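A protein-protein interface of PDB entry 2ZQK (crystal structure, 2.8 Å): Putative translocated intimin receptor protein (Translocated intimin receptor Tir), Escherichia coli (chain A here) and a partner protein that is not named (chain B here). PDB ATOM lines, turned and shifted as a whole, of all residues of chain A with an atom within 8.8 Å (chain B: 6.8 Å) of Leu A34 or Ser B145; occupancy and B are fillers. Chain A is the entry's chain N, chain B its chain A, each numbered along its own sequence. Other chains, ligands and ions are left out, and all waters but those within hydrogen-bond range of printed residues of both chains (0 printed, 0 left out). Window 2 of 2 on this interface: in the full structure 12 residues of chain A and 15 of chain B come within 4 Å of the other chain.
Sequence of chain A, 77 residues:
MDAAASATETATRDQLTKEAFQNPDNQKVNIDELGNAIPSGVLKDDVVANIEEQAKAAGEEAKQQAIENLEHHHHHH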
ATOM      1  N   ILE A  31     -13.209   6.105   8.525  1.00  0.00           N
ATOM      2  CA  ILE A  31     -13.397   6.143   7.087  1.00  0.00           C
ATOM      3  C   ILE A  31     -14.168   7.380   6.655  1.00  0.00           C
ATOM      4  O   ILE A  31     -15.278   7.624   7.129  1.00  0.00           O
ATOM      5  CB  ILE A  31     -14.118   4.902   6.612  1.00  0.00           C
ATOM      6  CG1 ILE A  31     -13.204   3.678   6.791  1.00  0.00           C
ATOM      7  CG2 ILE A  31     -14.587   5.094   5.170  1.00  0.00           C
ATOM      8  CD1 ILE A  31     -11.902   3.747   6.034  1.00  0.00           C
ATOM      9  N   ASP A  32     -13.561   8.162   5.757  1.00  0.00           N
ATOM     10  CA  ASP A  32     -14.159   9.394   5.250  1.00  0.00           C
ATOM     11  C   ASP A  32     -15.194   9.079   4.193  1.00  0.00           C
ATOM     12  O   ASP A  32     -15.341   7.927   3.780  1.00  0.00           O
ATOM     13  CB  ASP A  32     -13.089  10.321   4.675  1.00  0.00           C
ATOM     14  CG  ASP A  32     -12.485   9.795   3.392  1.00  0.00           C
ATOM     15  OD1 ASP A  32     -11.330  10.170   3.094  1.00  0.00           O
ATOM     16  OD2 ASP A  32     -13.159   9.024   2.673  1.00  0.00           O
ATOM     17  N   GLU A  33     -15.897  10.106   3.729  1.00  0.00           N
ATOM     18  CA  GLU A  33     -16.951   9.884   2.751  1.00  0.00           C
ATOM     19  C   GLU A  33     -16.497   9.356   1.403  1.00  0.00           C
ATOM     20  O   GLU A  33     -17.283   9.318   0.451  1.00  0.00           O
ATOM     21  CB  GLU A  33     -17.795  11.150   2.594  1.00  0.00           C
ATOM     22  CG  GLU A  33     -17.050  12.437   2.756  1.00  0.00           C
ATOM     23  CD  GLU A  33     -16.705  12.779   4.198  1.00  0.00           C
ATOM     24  OE1 GLU A  33     -17.565  13.346   4.918  1.00  0.00           O
ATOM     25  OE2 GLU A  33     -15.556  12.486   4.604  1.00  0.00           O
ATOM     26  N   LEU A  34     -15.244   8.909   1.336  1.00  0.00           N
ATOM     27  CA  LEU A  34     -14.684   8.392   0.090  1.00  0.00           C
ATOM     28  C   LEU A  34     -14.126   6.990   0.251  1.00  0.00           C
ATOM     29  O   LEU A  34     -13.433   6.484  -0.634  1.00  0.00           O
ATOM     30  CB  LEU A  34     -13.563   9.306  -0.431  1.00  0.00           C
ATOM     31  CG  LEU A  34     -13.818  10.771  -0.808  1.00  0.00           C
ATOM     32  CD1 LEU A  34     -12.496  11.364  -1.262  1.00  0.00           C
ATOM     33  CD2 LEU A  34     -14.856  10.901  -1.912  1.00  0.00           C
ATOM     34  N   GLY A  35     -14.427   6.357   1.377  1.00  0.00           N
ATOM     35  CA  GLY A  35     -13.931   5.012   1.610  1.00  0.00           C
ATOM     36  C   GLY A  35     -12.454   5.027   1.947  1.00  0.00           C
ATOM     37  O   GLY A  35     -11.785   4.001   1.861  1.00  0.00           O
ATOM     38  N   ASN A  36     -11.949   6.194   2.334  1.00  0.00           N
ATOM     39  CA  ASN A  36     -10.542   6.349   2.688  1.00  0.00           C
ATOM     40  C   ASN A  36     -10.295   6.373   4.180  1.00  0.00           C
ATOM     41  O   ASN A  36     -11.095   6.904   4.952  1.00  0.00           O
ATOM     42  CB  ASN A  36      -9.965   7.630   2.075  1.00  0.00           C
ATOM     43  CG  ASN A  36      -9.579   7.456   0.631  1.00  0.00           C
ATOM     44  OD1 ASN A  36      -9.773   8.358  -0.180  1.00  0.00           O
ATOM     45  ND2 ASN A  36      -9.025   6.291   0.298  1.00  0.00           N
ATOM     46  N   ALA A  37      -9.150   5.823   4.561  1.00  0.00           N
ATOM     47  CA  ALA A  37      -8.753   5.739   5.944  1.00  0.00           C
ATOM     48  C   ALA A  37      -8.377   7.073   6.513  1.00  0.00           C
ATOM     49  O   ALA A  37      -7.991   7.961   5.779  1.00  0.00           O
ATOM     50  CB  ALA A  37      -7.589   4.830   6.049  1.00  0.00           C
ATOM     51  N   ILE A  38      -8.502   7.222   7.824  1.00  0.00           N
ATOM     52  CA  ILE A  38      -8.067   8.445   8.498  1.00  0.00           C
ATOM     53  C   ILE A  38      -7.852   8.158   9.968  1.00  0.00           C
ATOM     54  O   ILE A  38      -8.498   7.282  10.541  1.00  0.00           O
ATOM     55  CB  ILE A  38      -9.062   9.650   8.409  1.00  0.00           C
ATOM     56  CG1 ILE A  38     -10.488   9.216   8.746  1.00  0.00           C
ATOM     57  CG2 ILE A  38      -8.951  10.309   7.071  1.00  0.00           C
ATOM     58  CD1 ILE A  38     -11.353  10.357   9.256  1.00  0.00           C
ATOM     59  N   GLN B 103     -25.926   3.246   6.582  1.00  0.00           N
ATOM     60  CA  GLN B 103     -24.599   3.326   7.162  1.00  0.00           C
ATOM     61  C   GLN B 103     -24.865   3.006   8.613  1.00  0.00           C
ATOM     62  O   GLN B 103     -25.920   3.364   9.131  1.00  0.00           O
ATOM     63  CB  GLN B 103     -24.043   4.733   7.035  1.00  0.00           C
ATOM     64  CG  GLN B 103     -24.145   5.261   5.631  1.00  0.00           C
ATOM     65  CD  GLN B 103     -23.039   6.238   5.305  1.00  0.00           C
ATOM     66  OE1 GLN B 103     -22.647   6.358   4.149  1.00  0.00           O
ATOM     67  NE2 GLN B 103     -22.529   6.943   6.323  1.00  0.00           N
ATOM     68  N   ASN B 135     -21.268   1.509  -8.893  1.00  0.00           N
ATOM     69  CA  ASN B 135     -21.798   2.748  -9.450  1.00  0.00           C
ATOM     70  C   ASN B 135     -21.913   2.706 -10.959  1.00  0.00           C
ATOM     71  O   ASN B 135     -22.398   3.653 -11.565  1.00  0.00           O
ATOM     72  CB  ASN B 135     -20.972   3.957  -9.020  1.00  0.00           C
ATOM     73  CG  ASN B 135     -19.520   3.829  -9.381  1.00  0.00           C
ATOM     74  OD1 ASN B 135     -18.673   4.498  -8.783  1.00  0.00           O
ATOM     75  ND2 ASN B 135     -19.216   2.974 -10.364  1.00  0.00           N
ATOM     76  N   SER B 142     -24.717   7.415  -9.069  1.00  0.00           N
ATOM     77  CA  SER B 142     -24.050   8.634  -8.640  1.00  0.00           C
ATOM     78  C   SER B 142     -23.398   8.542  -7.263  1.00  0.00           C
ATOM     79  O   SER B 142     -23.490   9.471  -6.452  1.00  0.00           O
ATOM     80  CB  SER B 142     -25.022   9.813  -8.659  1.00  0.00           C
ATOM     81  OG  SER B 142     -25.927   9.726  -7.579  1.00  0.00           O
ATOM     82  N   MET B 143     -22.736   7.423  -6.996  1.00  0.00           N
ATOM     83  CA  MET B 143     -22.052   7.270  -5.729  1.00  0.00           C
ATOM     84  C   MET B 143     -20.559   7.185  -5.996  1.00  0.00           C
ATOM     85  O   MET B 143     -20.136   6.651  -7.030  1.00  0.00           O
ATOM     86  CB  MET B 143     -22.541   6.023  -5.015  1.00  0.00           C
ATOM     87  CG  MET B 143     -23.952   6.153  -4.488  1.00  0.00           C
ATOM     88  SD  MET B 143     -24.458   4.637  -3.682  1.00  0.00           S
ATOM     89  CE  MET B 143     -23.937   4.948  -1.956  1.00  0.00           C
ATOM     90  N   ASN B 144     -19.768   7.733  -5.074  1.00  0.00           N
ATOM     91  CA  ASN B 144     -18.314   7.728  -5.205  1.00  0.00           C
ATOM     92  C   ASN B 144     -17.672   6.630  -4.367  1.00  0.00           C
ATOM     93  O   ASN B 144     -16.519   6.253  -4.594  1.00  0.00           O
ATOM     94  CB  ASN B 144     -17.738   9.087  -4.804  1.00  0.00           C
ATOM     95  CG  ASN B 144     -17.980  10.154  -5.852  1.00  0.00           C
ATOM     96  OD1 ASN B 144     -17.552  10.023  -7.001  1.00  0.00           O
ATOM     97  ND2 ASN B 144     -18.669  11.219  -5.463  1.00  0.00           N
ATOM     98  N   SER B 145     -18.428   6.132  -3.394  1.00  0.00           N
ATOM     99  CA  SER B 145     -17.959   5.069  -2.517  1.00  0.00           C
ATOM    100  C   SER B 145     -19.062   4.353  -1.764  1.00  0.00           C
ATOM    101  O   SER B 145     -20.119   4.916  -1.455  1.00  0.00           O
ATOM    102  CB  SER B 145     -16.979   5.601  -1.487  1.00  0.00           C
ATOM    103  OG  SER B 145     -16.682   4.578  -0.555  1.00  0.00           O
ATOM    104  N   ILE B 146     -18.774   3.096  -1.459  1.00  0.00           N
ATOM    105  CA  ILE B 146     -19.669   2.227  -0.711  1.00  0.00           C
ATOM    106  C   ILE B 146     -18.763   1.327   0.111  1.00  0.00           C
ATOM    107  O   ILE B 146     -18.536   0.184  -0.262  1.00  0.00           O
ATOM    108  CB  ILE B 146     -20.539   1.318  -1.639  1.00  0.00           C
ATOM    109  CG1 ILE B 146     -21.460   2.174  -2.524  1.00  0.00           C
ATOM    110  CG2 ILE B 146     -21.367   0.345  -0.788  1.00  0.00           C
ATOM    111  CD1 ILE B 146     -22.340   1.355  -3.455  1.00  0.00           C
ATOM    112  N   THR B 147     -18.206   1.847   1.199  1.00  0.00           N
ATOM    113  CA  THR B 147     -17.364   0.996   2.022  1.00  0.00           C
ATOM    114  C   THR B 147     -18.335   0.081   2.748  1.00  0.00           C
ATOM    115  O   THR B 147     -19.418   0.498   3.167  1.00  0.00           O
ATOM    116  CB  THR B 147     -16.519   1.775   3.050  1.00  0.00           C
ATOM    117  OG1 THR B 147     -15.698   2.745   2.382  1.00  0.00           O
ATOM    118  CG2 THR B 147     -15.609   0.813   3.786  1.00  0.00           C
ATOM    119  N   ASN B 166     -14.698  -2.249  -0.439  1.00  0.00           N
ATOM    120  CA  ASN B 166     -15.475  -1.192  -1.059  1.00  0.00           C
ATOM    121  C   ASN B 166     -16.181  -1.656  -2.324  1.00  0.00           C
ATOM    122  O   ASN B 166     -15.550  -1.900  -3.340  1.00  0.00           O
ATOM    123  CB  ASN B 166     -14.550  -0.003  -1.331  1.00  0.00           C
ATOM    124  CG  ASN B 166     -15.305   1.274  -1.606  1.00  0.00           C
ATOM    125  OD1 ASN B 166     -15.887   1.450  -2.683  1.00  0.00           O
ATOM    126  ND2 ASN B 166     -15.308   2.185  -0.627  1.00  0.00           N
ATOM    127  N   LEU B 167     -17.501  -1.778  -2.263  1.00  0.00           N
ATOM    128  CA  LEU B 167     -18.238  -2.235  -3.420  1.00  0.00           C
ATOM    129  C   LEU B 167     -17.972  -1.407  -4.653  1.00  0.00           C
ATOM    130  O   LEU B 167     -18.310  -1.817  -5.759  1.00  0.00           O
ATOM    131  CB  LEU B 167     -19.727  -2.284  -3.120  1.00  0.00           C
ATOM    132  CG  LEU B 167     -19.986  -3.351  -2.054  1.00  0.00           C
ATOM    133  CD1 LEU B 167     -21.494  -3.459  -1.788  1.00  0.00           C
ATOM    134  CD2 LEU B 167     -19.386  -4.690  -2.514  1.00  0.00           C
ATOM    135  N   ILE B 168     -17.379  -0.234  -4.489  1.00  0.00           N
ATOM    136  CA  ILE B 168     -17.069   0.542  -5.664  1.00  0.00           C
ATOM    137  C   ILE B 168     -15.577   0.566  -5.958  1.00  0.00           C
ATOM    138  O   ILE B 168     -15.139   0.054  -6.976  1.00  0.00           O
ATOM    139  CB  ILE B 168     -17.552   1.981  -5.565  1.00  0.00           C
ATOM    140  CG1 ILE B 168     -19.085   2.018  -5.667  1.00  0.00           C
ATOM    141  CG2 ILE B 168     -16.873   2.824  -6.703  1.00  0.00           C
ATOM    142  CD1 ILE B 168     -19.700   3.371  -5.371  1.00  0.00           C
ATOM    143  N   THR B 169     -14.792   1.129  -5.056  1.00  0.00           N
ATOM    144  CA  THR B 169     -13.361   1.243  -5.275  1.00  0.00           C
ATOM    145  C   THR B 169     -12.521   0.083  -4.755  1.00  0.00           C
ATOM    146  O   THR B 169     -11.294   0.141  -4.805  1.00  0.00           O
ATOM    147  CB  THR B 169     -12.829   2.519  -4.625  1.00  0.00           C
ATOM    148  OG1 THR B 169     -12.605   2.280  -3.228  1.00  0.00           O
ATOM    149  CG2 THR B 169     -13.831   3.675  -4.784  1.00  0.00           C
ATOM    150  N   ASN B 171     -10.496  -1.285  -2.604  1.00  0.00           N
ATOM    151  CA  ASN B 171      -9.688  -0.791  -1.496  1.00  0.00           C
ATOM    152  C   ASN B 171      -9.984  -1.422  -0.124  1.00  0.00           C
ATOM    153  O   ASN B 171     -10.538  -0.780   0.762  1.00  0.00           O
ATOM    154  CB  ASN B 171      -9.852   0.733  -1.438  1.00  0.00           C
ATOM    155  CG  ASN B 171      -9.194   1.359  -0.221  1.00  0.00           C
ATOM    156  OD1 ASN B 171      -8.074   1.001   0.155  1.00  0.00           O
ATOM    157  ND2 ASN B 171      -9.882   2.316   0.390  1.00  0.00           N
ATOM    158  N   ASN B 182     -19.675   6.458   7.752  1.00  0.00           N
ATOM    159  CA  ASN B 182     -19.295   6.139   6.375  1.00  0.00           C
ATOM    160  C   ASN B 182     -19.033   4.686   6.017  1.00  0.00           C
ATOM    161  O   ASN B 182     -18.274   4.412   5.090  1.00  0.00           O
ATOM    162  CB  ASN B 182     -18.073   6.976   5.944  1.00  0.00           C
ATOM    163  CG  ASN B 182     -18.371   8.456   5.932  1.00  0.00           C
ATOM    164  OD1 ASN B 182     -17.874   9.219   6.765  1.00  0.00           O
ATOM    165  ND2 ASN B 182     -19.217   8.870   4.989  1.00  0.00           N
ATOM    166  N   TYR B 184     -21.230   1.214   5.161  1.00  0.00           N
ATOM    167  CA  TYR B 184     -22.564   0.670   4.922  1.00  0.00           C
ATOM    168  C   TYR B 184     -22.774  -0.731   5.447  1.00  0.00           C
ATOM    169  O   TYR B 184     -21.865  -1.561   5.429  1.00  0.00           O
ATOM    170  CB  TYR B 184     -22.883   0.669   3.432  1.00  0.00           C
ATOM    171  CG  TYR B 184     -23.094   2.035   2.832  1.00  0.00           C
ATOM    172  CD1 TYR B 184     -22.018   2.861   2.545  1.00  0.00           C
ATOM    173  CD2 TYR B 184     -24.374   2.502   2.556  1.00  0.00           C
ATOM    174  CE1 TYR B 184     -22.203   4.121   2.000  1.00  0.00           C
ATOM    175  CE2 TYR B 184     -24.573   3.757   2.009  1.00  0.00           C
ATOM    176  CZ  TYR B 184     -23.479   4.567   1.734  1.00  0.00           C
ATOM    177  OH  TYR B 184     -23.659   5.821   1.202  1.00  0.00           O
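The backbone NH (N) of Gly A35 sits at hydrogen-bond distance from the side-chain hydroxyl (OG) of Ser B145, at 3.5 Å. ND2 of Asn B171 is in hydrogen-bond range of O of Gly A35 (2.9 Å). The side-chain amide oxygen (OD1) of Asn B182 lies close to the backbone carbonyl oxygen (O) of Ile A31 (3.1 Å).
The side-chain hydroxyl (OG) of Ser B145 is in hydrogen-bond range of the side-chain amide nitrogen (ND2) of Asn B166, at 2.8 Å. The side-chain amide nitrogen of Asn B166 lies within hydrogen-bond range of the side-chain hydroxyl of Thr B147 (3.1 Å). The backbone NH (N) of Tyr B184 sits at hydrogen-bond distance from the backbone carbonyl oxygen (O) of Thr B147, 2.8 Å away. The side-chain amide oxygen (OD1) of Asn B166 is in hydrogen-bond range of the backbone NH (N) of Thr B169, 2.6 Å away. OD2 of Asp A32 is in hydrogen-bond range of N of Leu A34. The side-chain carboxylate (OD2) of Asp A32 is in hydrogen-bond range of the backbone NH (N) of Asn A36, 3.1 Å away.
Among the printed residues, pairs that only touch across the chains: Gly A35 with Thr B147 (3.0 Å), Glu A33 with Asn B182 (3.3 Å), Leu A34 with Ser B145 (3.6 Å), Asp A32 with Asn B182 (3.6 Å), Ile A31 with Thr B147 (3.8 Å) and Gly A35 with Asn B166 (3.9 Å).
Of chain A, only Leu A34 and Gly A35 come within 4 Å of Ser B145. No residue of chain A comes within 4 Å of Ile B146. Of the printed residues of chain B, Asp A32 touches Asn B182 (3.6 Å). Of the printed residues of chain A, Asn B182 touches Ile A31 (3.1 Å), Asp A32 (3.6 Å) and Glu A33 (3.3 Å). Of the printed residues of chain A, Asn B171 touches Gly A35 (2.9 Å). Printed residues of chain A within 4 Å of Asn B166: Gly A35. Printed residues of chain B within 4 Å of Ile A31: Thr B147 and Asn B182. The nearest residue of chain B that does not touch Leu A34 is Asn B144 (4.5 Å). The nearest residue of chain A that does not touch Ser B145 is Glu A33 (4.2 Å).
Printed residues of chain A that touch a printed residue of chain B: Ile A31, Asp A32, Glu A33, Leu A34 and Gly A35. Hydrophobic or aromatic side chains of chain A within 4 Å of the printed part of chain B: Ile A31. Among the printed residues, 9 pairs touch across the chains. Among the printed residues, no Asp or Glu carboxylate lies within 4 Å of a Lys or Arg side-chain nitrogen of the other chain.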
